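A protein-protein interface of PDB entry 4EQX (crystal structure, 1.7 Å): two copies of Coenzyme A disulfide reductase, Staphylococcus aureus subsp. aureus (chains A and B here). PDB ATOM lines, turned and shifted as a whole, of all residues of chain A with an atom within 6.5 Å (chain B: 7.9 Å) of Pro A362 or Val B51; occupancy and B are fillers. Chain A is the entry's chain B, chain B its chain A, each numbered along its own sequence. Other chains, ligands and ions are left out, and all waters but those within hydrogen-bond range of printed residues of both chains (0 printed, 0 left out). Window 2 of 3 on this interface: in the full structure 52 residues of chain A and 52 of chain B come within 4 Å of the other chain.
The backbone carbonyl oxygen of Tyr B46 lies within hydrogen-bond range of the backbone NH of Val B51 (3.0 Å). O of Tyr B46 lies within hydrogen-bond range of N of Val B52 (3.2 Å). NZ of Lys B326 lies within salt-bridge range of OE2 of Glu B164. A ring nitrogen (NE2) of His A357 sits at hydrogen-bond distance from the backbone carbonyl oxygen (O) of Tyr A361 (3.1 Å). O of Pro A362 sits at hydrogen-bond distance from NE2 of His A357 (2.9 Å).
The backbone NH (N) of Ala B43 lies within hydrogen-bond range of the side-chain hydroxyl (OH) of Tyr A360 (3.3 Å).
No position is printed for both chains.
Among the printed residues, pairs that only touch across the chains: Asn A359 with Tyr B57, Tyr A360 with Val B52, Tyr A360 with Tyr B57, Tyr A361 with Tyr B46, Tyr A361 with Lys B326 and Pro A362 with Val B51.
Of the 17 printed residues of chain B, 6 touch a printed residue of chain A. Printed residues of chain A that touch a printed residue of chain B: Asn A359, Tyr A360, Tyr A361 and Pro A362. Among the printed residues, no Asp or Glu carboxylate lies within 4 Å of a Lys or Arg side-chain nitrogen of the other chain.
Val B51 touches one residue of chain A. Printed residues of chain A within 4 Å of Lys B326: Tyr A361. Printed residues of chain A within 4 Å of Val B52: Tyr A360. The nearest residue of chain A that does not touch Val B51 is Tyr A361 (4.4 Å). The nearest printed residue of chain B that does not touch Tyr A361 is Val B51 (4.4 Å).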
ATOM      1  N   HIS A 357       3.264   1.007 -21.425  1.00  0.00           N
ATOM      2  CA  HIS A 357       2.192   1.911 -20.896  1.00  0.00           C
ATOM      3  C   HIS A 357       1.845   1.310 -19.546  1.00  0.00           C
ATOM      4  O   HIS A 357       2.578   0.418 -19.081  1.00  0.00           O
ATOM      5  CB  HIS A 357       0.995   1.969 -21.868  1.00  0.00           C
ATOM      6  CG  HIS A 357       0.379   0.643 -22.157  1.00  0.00           C
ATOM      7  ND1 HIS A 357       0.192   0.156 -23.439  1.00  0.00           N
ATOM      8  CD2 HIS A 357      -0.106  -0.303 -21.312  1.00  0.00           C
ATOM      9  CE1 HIS A 357      -0.417  -1.014 -23.363  1.00  0.00           C
ATOM     10  NE2 HIS A 357      -0.594  -1.311 -22.089  1.00  0.00           N
ATOM     11  N   ALA A 358       0.749   1.756 -18.905  1.00  0.00           N
ATOM     12  CA  ALA A 358       0.690   1.558 -17.440  1.00  0.00           C
ATOM     13  C   ALA A 358       0.620   0.060 -17.147  1.00  0.00           C
ATOM     14  O   ALA A 358      -0.060  -0.680 -17.848  1.00  0.00           O
ATOM     15  CB  ALA A 358      -0.553   2.245 -16.863  1.00  0.00           C
ATOM     16  N   ASN A 359       1.314  -0.325 -16.068  1.00  0.00           N
ATOM     17  CA  ASN A 359       1.445  -1.724 -15.658  1.00  0.00           C
ATOM     18  C   ASN A 359       0.214  -2.530 -15.576  1.00  0.00           C
ATOM     19  O   ASN A 359       0.259  -3.736 -15.837  1.00  0.00           O
ATOM     20  CB  ASN A 359       2.080  -1.779 -14.288  1.00  0.00           C
ATOM     21  CG  ASN A 359       3.536  -1.804 -14.399  1.00  0.00           C
ATOM     22  OD1 ASN A 359       4.079  -2.793 -14.929  1.00  0.00           O
ATOM     23  ND2 ASN A 359       4.216  -0.690 -14.003  1.00  0.00           N
ATOM     24  N   TYR A 360      -0.857  -1.859 -15.142  1.00  0.00           N
ATOM     25  CA  TYR A 360      -2.189  -2.457 -14.962  1.00  0.00           C
ATOM     26  C   TYR A 360      -3.021  -2.533 -16.210  1.00  0.00           C
ATOM     27  O   TYR A 360      -4.065  -3.186 -16.212  1.00  0.00           O
ATOM     28  CB  TYR A 360      -3.010  -1.663 -13.907  1.00  0.00           C
ATOM     29  CG  TYR A 360      -3.084  -0.139 -14.095  1.00  0.00           C
ATOM     30  CD1 TYR A 360      -3.964   0.422 -15.008  1.00  0.00           C
ATOM     31  CD2 TYR A 360      -2.267   0.712 -13.337  1.00  0.00           C
ATOM     32  CE1 TYR A 360      -4.049   1.805 -15.193  1.00  0.00           C
ATOM     33  CE2 TYR A 360      -2.329   2.120 -13.510  1.00  0.00           C
ATOM     34  CZ  TYR A 360      -3.222   2.619 -14.459  1.00  0.00           C
ATOM     35  OH  TYR A 360      -3.309   3.959 -14.609  1.00  0.00           O
ATOM     36  N   TYR A 361      -2.624  -1.741 -17.222  1.00  0.00           N
ATOM     37  CA  TYR A 361      -3.441  -1.525 -18.385  1.00  0.00           C
ATOM     38  C   TYR A 361      -3.102  -2.566 -19.405  1.00  0.00           C
ATOM     39  O   TYR A 361      -1.906  -2.761 -19.675  1.00  0.00           O
ATOM     40  CB  TYR A 361      -3.130  -0.137 -18.992  1.00  0.00           C
ATOM     41  CG  TYR A 361      -4.096   0.202 -20.103  1.00  0.00           C
ATOM     42  CD1 TYR A 361      -5.331   0.795 -19.794  1.00  0.00           C
ATOM     43  CD2 TYR A 361      -3.792  -0.063 -21.446  1.00  0.00           C
ATOM     44  CE1 TYR A 361      -6.281   1.091 -20.818  1.00  0.00           C
ATOM     45  CE2 TYR A 361      -4.703   0.288 -22.487  1.00  0.00           C
ATOM     46  CZ  TYR A 361      -5.931   0.895 -22.126  1.00  0.00           C
ATOM     47  OH  TYR A 361      -6.847   1.199 -23.064  1.00  0.00           O
ATOM     48  N   PRO A 362      -4.111  -3.158 -20.060  1.00  0.00           N
ATOM     49  CA  PRO A 362      -3.979  -4.399 -20.838  1.00  0.00           C
ATOM     50  C   PRO A 362      -3.097  -4.251 -22.040  1.00  0.00           C
ATOM     51  O   PRO A 362      -2.820  -3.123 -22.435  1.00  0.00           O
ATOM     52  CB  PRO A 362      -5.386  -4.680 -21.345  1.00  0.00           C
ATOM     53  CG  PRO A 362      -6.287  -3.639 -20.795  1.00  0.00           C
ATOM     54  CD  PRO A 362      -5.447  -2.560 -20.176  1.00  0.00           C
ATOM     55  N   GLY A 363      -2.672  -5.378 -22.637  1.00  0.00           N
ATOM     56  CA  GLY A 363      -2.121  -5.304 -23.996  1.00  0.00           C
ATOM     57  C   GLY A 363      -0.693  -4.823 -23.932  1.00  0.00           C
ATOM     58  O   GLY A 363      -0.151  -4.386 -24.931  1.00  0.00           O
ATOM     59  N   ASN A 364      -0.095  -4.929 -22.753  1.00  0.00           N
ATOM     60  CA  ASN A 364       1.173  -4.272 -22.459  1.00  0.00           C
ATOM     61  C   ASN A 364       2.243  -5.166 -23.044  1.00  0.00           C
ATOM     62  O   ASN A 364       1.938  -6.297 -23.425  1.00  0.00           O
ATOM     63  CB  ASN A 364       1.395  -4.074 -20.969  1.00  0.00           C
ATOM     64  CG  ASN A 364       2.292  -2.819 -20.620  1.00  0.00           C
ATOM     65  OD1 ASN A 364       2.710  -1.993 -21.495  1.00  0.00           O
ATOM     66  ND2 ASN A 364       2.552  -2.659 -19.333  1.00  0.00           N
ATOM     67  N   GLU A 389       5.781  -2.290 -28.533  1.00  0.00           N
ATOM     68  CA  GLU A 389       5.080  -1.020 -28.428  1.00  0.00           C
ATOM     69  C   GLU A 389       6.012   0.069 -27.895  1.00  0.00           C
ATOM     70  O   GLU A 389       6.778  -0.172 -26.917  1.00  0.00           O
ATOM     71  CB  GLU A 389       3.936  -1.220 -27.415  1.00  0.00           C
ATOM     72  CG  GLU A 389       3.126   0.092 -27.179  1.00  0.00           C
ATOM     73  CD  GLU A 389       1.817  -0.081 -26.365  1.00  0.00           C
ATOM     74  OE1 GLU A 389       1.386   0.907 -25.713  1.00  0.00           O
ATOM     75  OE2 GLU A 389       1.207  -1.160 -26.415  1.00  0.00           O
ATOM     76  N   ALA B  43      -6.205   4.440 -13.058  1.00  0.00           N
ATOM     77  CA  ALA B  43      -6.792   3.181 -13.456  1.00  0.00           C
ATOM     78  C   ALA B  43      -8.260   3.115 -13.154  1.00  0.00           C
ATOM     79  O   ALA B  43      -8.944   2.177 -13.644  1.00  0.00           O
ATOM     80  CB  ALA B  43      -6.096   2.006 -12.696  1.00  0.00           C
ATOM     81  N   PRO B  45     -11.208   4.544 -13.988  1.00  0.00           N
ATOM     82  CA  PRO B  45     -12.256   4.344 -14.974  1.00  0.00           C
ATOM     83  C   PRO B  45     -12.222   2.944 -15.569  1.00  0.00           C
ATOM     84  O   PRO B  45     -13.243   2.376 -15.881  1.00  0.00           O
ATOM     85  CB  PRO B  45     -11.924   5.460 -16.056  1.00  0.00           C
ATOM     86  CG  PRO B  45     -11.237   6.606 -15.254  1.00  0.00           C
ATOM     87  CD  PRO B  45     -10.373   5.753 -14.315  1.00  0.00           C
ATOM     88  N   TYR B  46     -11.030   2.419 -15.820  1.00  0.00           N
ATOM     89  CA  TYR B  46     -10.807   1.066 -16.403  1.00  0.00           C
ATOM     90  C   TYR B  46     -11.201  -0.024 -15.467  1.00  0.00           C
ATOM     91  O   TYR B  46     -11.665  -1.088 -15.927  1.00  0.00           O
ATOM     92  CB  TYR B  46      -9.337   0.931 -16.877  1.00  0.00           C
ATOM     93  CG  TYR B  46      -9.040   2.069 -17.860  1.00  0.00           C
ATOM     94  CD1 TYR B  46      -8.408   3.248 -17.441  1.00  0.00           C
ATOM     95  CD2 TYR B  46      -9.460   1.988 -19.140  1.00  0.00           C
ATOM     96  CE1 TYR B  46      -8.119   4.307 -18.318  1.00  0.00           C
ATOM     97  CE2 TYR B  46      -9.252   3.061 -20.044  1.00  0.00           C
ATOM     98  CZ  TYR B  46      -8.590   4.188 -19.645  1.00  0.00           C
ATOM     99  OH  TYR B  46      -8.469   5.139 -20.605  1.00  0.00           O
ATOM    100  N   VAL B  47     -11.124   0.242 -14.163  1.00  0.00           N
ATOM    101  CA  VAL B  47     -11.653  -0.732 -13.187  1.00  0.00           C
ATOM    102  C   VAL B  47     -13.186  -0.758 -13.307  1.00  0.00           C
ATOM    103  O   VAL B  47     -13.829  -1.853 -13.355  1.00  0.00           O
ATOM    104  CB  VAL B  47     -11.262  -0.389 -11.775  1.00  0.00           C
ATOM    105  CG1 VAL B  47     -12.016  -1.295 -10.787  1.00  0.00           C
ATOM    106  CG2 VAL B  47      -9.725  -0.456 -11.556  1.00  0.00           C
ATOM    107  N   ILE B  48     -13.818   0.420 -13.398  1.00  0.00           N
ATOM    108  CA  ILE B  48     -15.291   0.417 -13.661  1.00  0.00           C
ATOM    109  C   ILE B  48     -15.670  -0.330 -14.940  1.00  0.00           C
ATOM    110  O   ILE B  48     -16.703  -1.031 -14.959  1.00  0.00           O
ATOM    111  CB  ILE B  48     -15.813   1.868 -13.717  1.00  0.00           C
ATOM    112  CG1 ILE B  48     -15.690   2.470 -12.281  1.00  0.00           C
ATOM    113  CG2 ILE B  48     -17.283   1.927 -14.244  1.00  0.00           C
ATOM    114  CD1 ILE B  48     -15.828   3.972 -12.221  1.00  0.00           C
ATOM    115  N   GLY B  49     -14.824  -0.226 -16.001  1.00  0.00           N
ATOM    116  CA  GLY B  49     -15.144  -0.872 -17.313  1.00  0.00           C
ATOM    117  C   GLY B  49     -14.805  -2.337 -17.330  1.00  0.00           C
ATOM    118  O   GLY B  49     -15.056  -3.035 -18.335  1.00  0.00           O
ATOM    119  N   GLU B  50     -14.272  -2.786 -16.189  1.00  0.00           N
ATOM    120  CA  GLU B  50     -13.743  -4.151 -16.086  1.00  0.00           C
ATOM    121  C   GLU B  50     -12.690  -4.467 -17.148  1.00  0.00           C
ATOM    122  O   GLU B  50     -12.547  -5.645 -17.510  1.00  0.00           O
ATOM    123  CB  GLU B  50     -14.888  -5.155 -16.221  1.00  0.00           C
ATOM    124  CG  GLU B  50     -15.666  -5.360 -14.984  1.00  0.00           C
ATOM    125  CD  GLU B  50     -17.070  -5.933 -15.217  1.00  0.00           C
ATOM    126  OE1 GLU B  50     -17.800  -6.023 -14.232  1.00  0.00           O
ATOM    127  OE2 GLU B  50     -17.467  -6.259 -16.356  1.00  0.00           O
ATOM    128  N   VAL B  51     -11.977  -3.458 -17.656  1.00  0.00           N
ATOM    129  CA  VAL B  51     -10.858  -3.549 -18.606  1.00  0.00           C
ATOM    130  C   VAL B  51      -9.583  -3.870 -17.786  1.00  0.00           C
ATOM    131  O   VAL B  51      -8.664  -4.620 -18.242  1.00  0.00           O
ATOM    132  CB  VAL B  51     -10.737  -2.233 -19.413  1.00  0.00           C
ATOM    133  CG1 VAL B  51      -9.304  -1.920 -19.969  1.00  0.00           C
ATOM    134  CG2 VAL B  51     -11.747  -2.207 -20.563  1.00  0.00           C
ATOM    135  N   VAL B  52      -9.504  -3.295 -16.584  1.00  0.00           N
ATOM    136  CA  VAL B  52      -8.621  -3.790 -15.542  1.00  0.00           C
ATOM    137  C   VAL B  52      -9.535  -4.720 -14.725  1.00  0.00           C
ATOM    138  O   VAL B  52     -10.427  -4.242 -13.988  1.00  0.00           O
ATOM    139  CB  VAL B  52      -8.088  -2.606 -14.654  1.00  0.00           C
ATOM    140  CG1 VAL B  52      -7.479  -3.116 -13.356  1.00  0.00           C
ATOM    141  CG2 VAL B  52      -7.144  -1.732 -15.419  1.00  0.00           C
ATOM    142  N   GLU B  53      -9.333  -6.038 -14.836  1.00  0.00           N
ATOM    143  CA  GLU B  53     -10.192  -7.045 -14.129  1.00  0.00           C
ATOM    144  C   GLU B  53      -9.785  -7.248 -12.672  1.00  0.00           C
ATOM    145  O   GLU B  53     -10.633  -7.344 -11.767  1.00  0.00           O
ATOM    146  CB  GLU B  53     -10.147  -8.462 -14.808  1.00  0.00           C
ATOM    147  CG  GLU B  53     -11.139  -8.767 -15.980  1.00  0.00           C
ATOM    148  CD  GLU B  53     -12.692  -8.883 -15.610  1.00  0.00           C
ATOM    149  OE1 GLU B  53     -13.465  -9.308 -16.495  1.00  0.00           O
ATOM    150  OE2 GLU B  53     -13.173  -8.560 -14.488  1.00  0.00           O
ATOM    151  N   ASP B  54      -8.479  -7.400 -12.476  1.00  0.00           N
ATOM    152  CA  ASP B  54      -7.908  -7.798 -11.183  1.00  0.00           C
ATOM    153  C   ASP B  54      -7.718  -6.484 -10.336  1.00  0.00           C
ATOM    154  O   ASP B  54      -6.683  -5.814 -10.434  1.00  0.00           O
ATOM    155  CB  ASP B  54      -6.673  -8.748 -11.485  1.00  0.00           C
ATOM    156  CG  ASP B  54      -5.422  -8.530 -10.573  1.00  0.00           C
ATOM    157  OD1 ASP B  54      -4.427  -7.929 -11.110  1.00  0.00           O
ATOM    158  OD2 ASP B  54      -5.412  -9.006  -9.387  1.00  0.00           O
ATOM    159  N   TYR B  57      -4.819  -4.811  -9.149  1.00  0.00           N
ATOM    160  CA  TYR B  57      -3.989  -4.060 -10.124  1.00  0.00           C
ATOM    161  C   TYR B  57      -3.982  -2.549  -9.854  1.00  0.00           C
ATOM    162  O   TYR B  57      -3.015  -1.883 -10.161  1.00  0.00           O
ATOM    163  CB  TYR B  57      -4.557  -4.224 -11.545  1.00  0.00           C
ATOM    164  CG  TYR B  57      -3.736  -5.049 -12.518  1.00  0.00           C
ATOM    165  CD1 TYR B  57      -4.392  -5.840 -13.492  1.00  0.00           C
ATOM    166  CD2 TYR B  57      -2.304  -5.034 -12.488  1.00  0.00           C
ATOM    167  CE1 TYR B  57      -3.660  -6.601 -14.422  1.00  0.00           C
ATOM    168  CE2 TYR B  57      -1.557  -5.810 -13.412  1.00  0.00           C
ATOM    169  CZ  TYR B  57      -2.255  -6.591 -14.381  1.00  0.00           C
ATOM    170  OH  TYR B  57      -1.569  -7.367 -15.307  1.00  0.00           O
ATOM    171  N   GLU B 164     -16.772   5.788 -21.812  1.00  0.00           N
ATOM    172  CA  GLU B 164     -16.271   4.739 -22.660  1.00  0.00           C
ATOM    173  C   GLU B 164     -16.300   3.392 -21.887  1.00  0.00           C
ATOM    174  O   GLU B 164     -16.826   2.359 -22.406  1.00  0.00           O
ATOM    175  CB  GLU B 164     -14.875   5.067 -23.206  1.00  0.00           C
ATOM    176  CG  GLU B 164     -14.239   3.795 -23.836  1.00  0.00           C
ATOM    177  CD  GLU B 164     -13.089   4.092 -24.764  1.00  0.00           C
ATOM    178  OE1 GLU B 164     -12.435   5.126 -24.649  1.00  0.00           O
ATOM    179  OE2 GLU B 164     -12.825   3.189 -25.616  1.00  0.00           O
ATOM    180  N   ASN B 165     -15.778   3.384 -20.659  1.00  0.00           N
ATOM    181  CA  ASN B 165     -15.738   2.162 -19.908  1.00  0.00           C
ATOM    182  C   ASN B 165     -17.135   1.595 -19.575  1.00  0.00           C
ATOM    183  O   ASN B 165     -17.354   0.346 -19.580  1.00  0.00           O
ATOM    184  CB  ASN B 165     -14.942   2.361 -18.667  1.00  0.00           C
ATOM    185  CG  ASN B 165     -13.465   2.152 -18.934  1.00  0.00           C
ATOM    186  OD1 ASN B 165     -13.011   1.004 -18.991  1.00  0.00           O
ATOM    187  ND2 ASN B 165     -12.739   3.240 -19.115  1.00  0.00           N
ATOM    188  N   GLU B 168     -18.309  -0.010 -22.723  1.00  0.00           N
ATOM    189  CA  GLU B 168     -17.694  -1.324 -23.012  1.00  0.00           C
ATOM    190  C   GLU B 168     -18.193  -2.423 -22.052  1.00  0.00           C
ATOM    191  O   GLU B 168     -18.314  -3.636 -22.462  1.00  0.00           O
ATOM    192  CB  GLU B 168     -16.166  -1.204 -23.035  1.00  0.00           C
ATOM    193  CG  GLU B 168     -15.678  -0.355 -24.214  1.00  0.00           C
ATOM    194  CD  GLU B 168     -16.093  -0.805 -25.655  1.00  0.00           C
ATOM    195  OE1 GLU B 168     -15.798  -0.044 -26.586  1.00  0.00           O
ATOM    196  OE2 GLU B 168     -16.740  -1.869 -25.909  1.00  0.00           O
ATOM    197  N   ARG B 169     -18.465  -2.029 -20.805  1.00  0.00           N
ATOM    198  CA  ARG B 169     -18.980  -2.980 -19.859  1.00  0.00           C
ATOM    199  C   ARG B 169     -20.376  -3.484 -20.280  1.00  0.00           C
ATOM    200  O   ARG B 169     -20.886  -4.506 -19.694  1.00  0.00           O
ATOM    201  CB  ARG B 169     -18.993  -2.361 -18.446  1.00  0.00           C
ATOM    202  CG  ARG B 169     -19.693  -3.209 -17.365  1.00  0.00           C
ATOM    203  CD  ARG B 169     -19.318  -2.605 -16.049  1.00  0.00           C
ATOM    204  NE  ARG B 169     -19.939  -3.285 -14.909  1.00  0.00           N
ATOM    205  CZ  ARG B 169     -19.538  -3.231 -13.641  1.00  0.00           C
ATOM    206  NH1 ARG B 169     -18.521  -2.458 -13.210  1.00  0.00           N
ATOM    207  NH2 ARG B 169     -20.208  -3.945 -12.727  1.00  0.00           N
ATOM    208  N   LYS B 326      -7.377   8.993 -24.362  1.00  0.00           N
ATOM    209  CA  LYS B 326      -7.961   8.067 -25.324  1.00  0.00           C
ATOM    210  C   LYS B 326      -9.457   8.156 -25.240  1.00  0.00           C
ATOM    211  O   LYS B 326     -10.023   8.137 -24.126  1.00  0.00           O
ATOM    212  CB  LYS B 326      -7.475   6.657 -24.961  1.00  0.00           C
ATOM    213  CG  LYS B 326      -7.949   5.577 -25.915  1.00  0.00           C
ATOM    214  CD  LYS B 326      -7.914   4.244 -25.092  1.00  0.00           C
ATOM    215  CE  LYS B 326      -9.183   3.291 -25.171  1.00  0.00           C
ATOM    216  NZ  LYS B 326     -10.035   3.232 -26.397  1.00  0.00           N
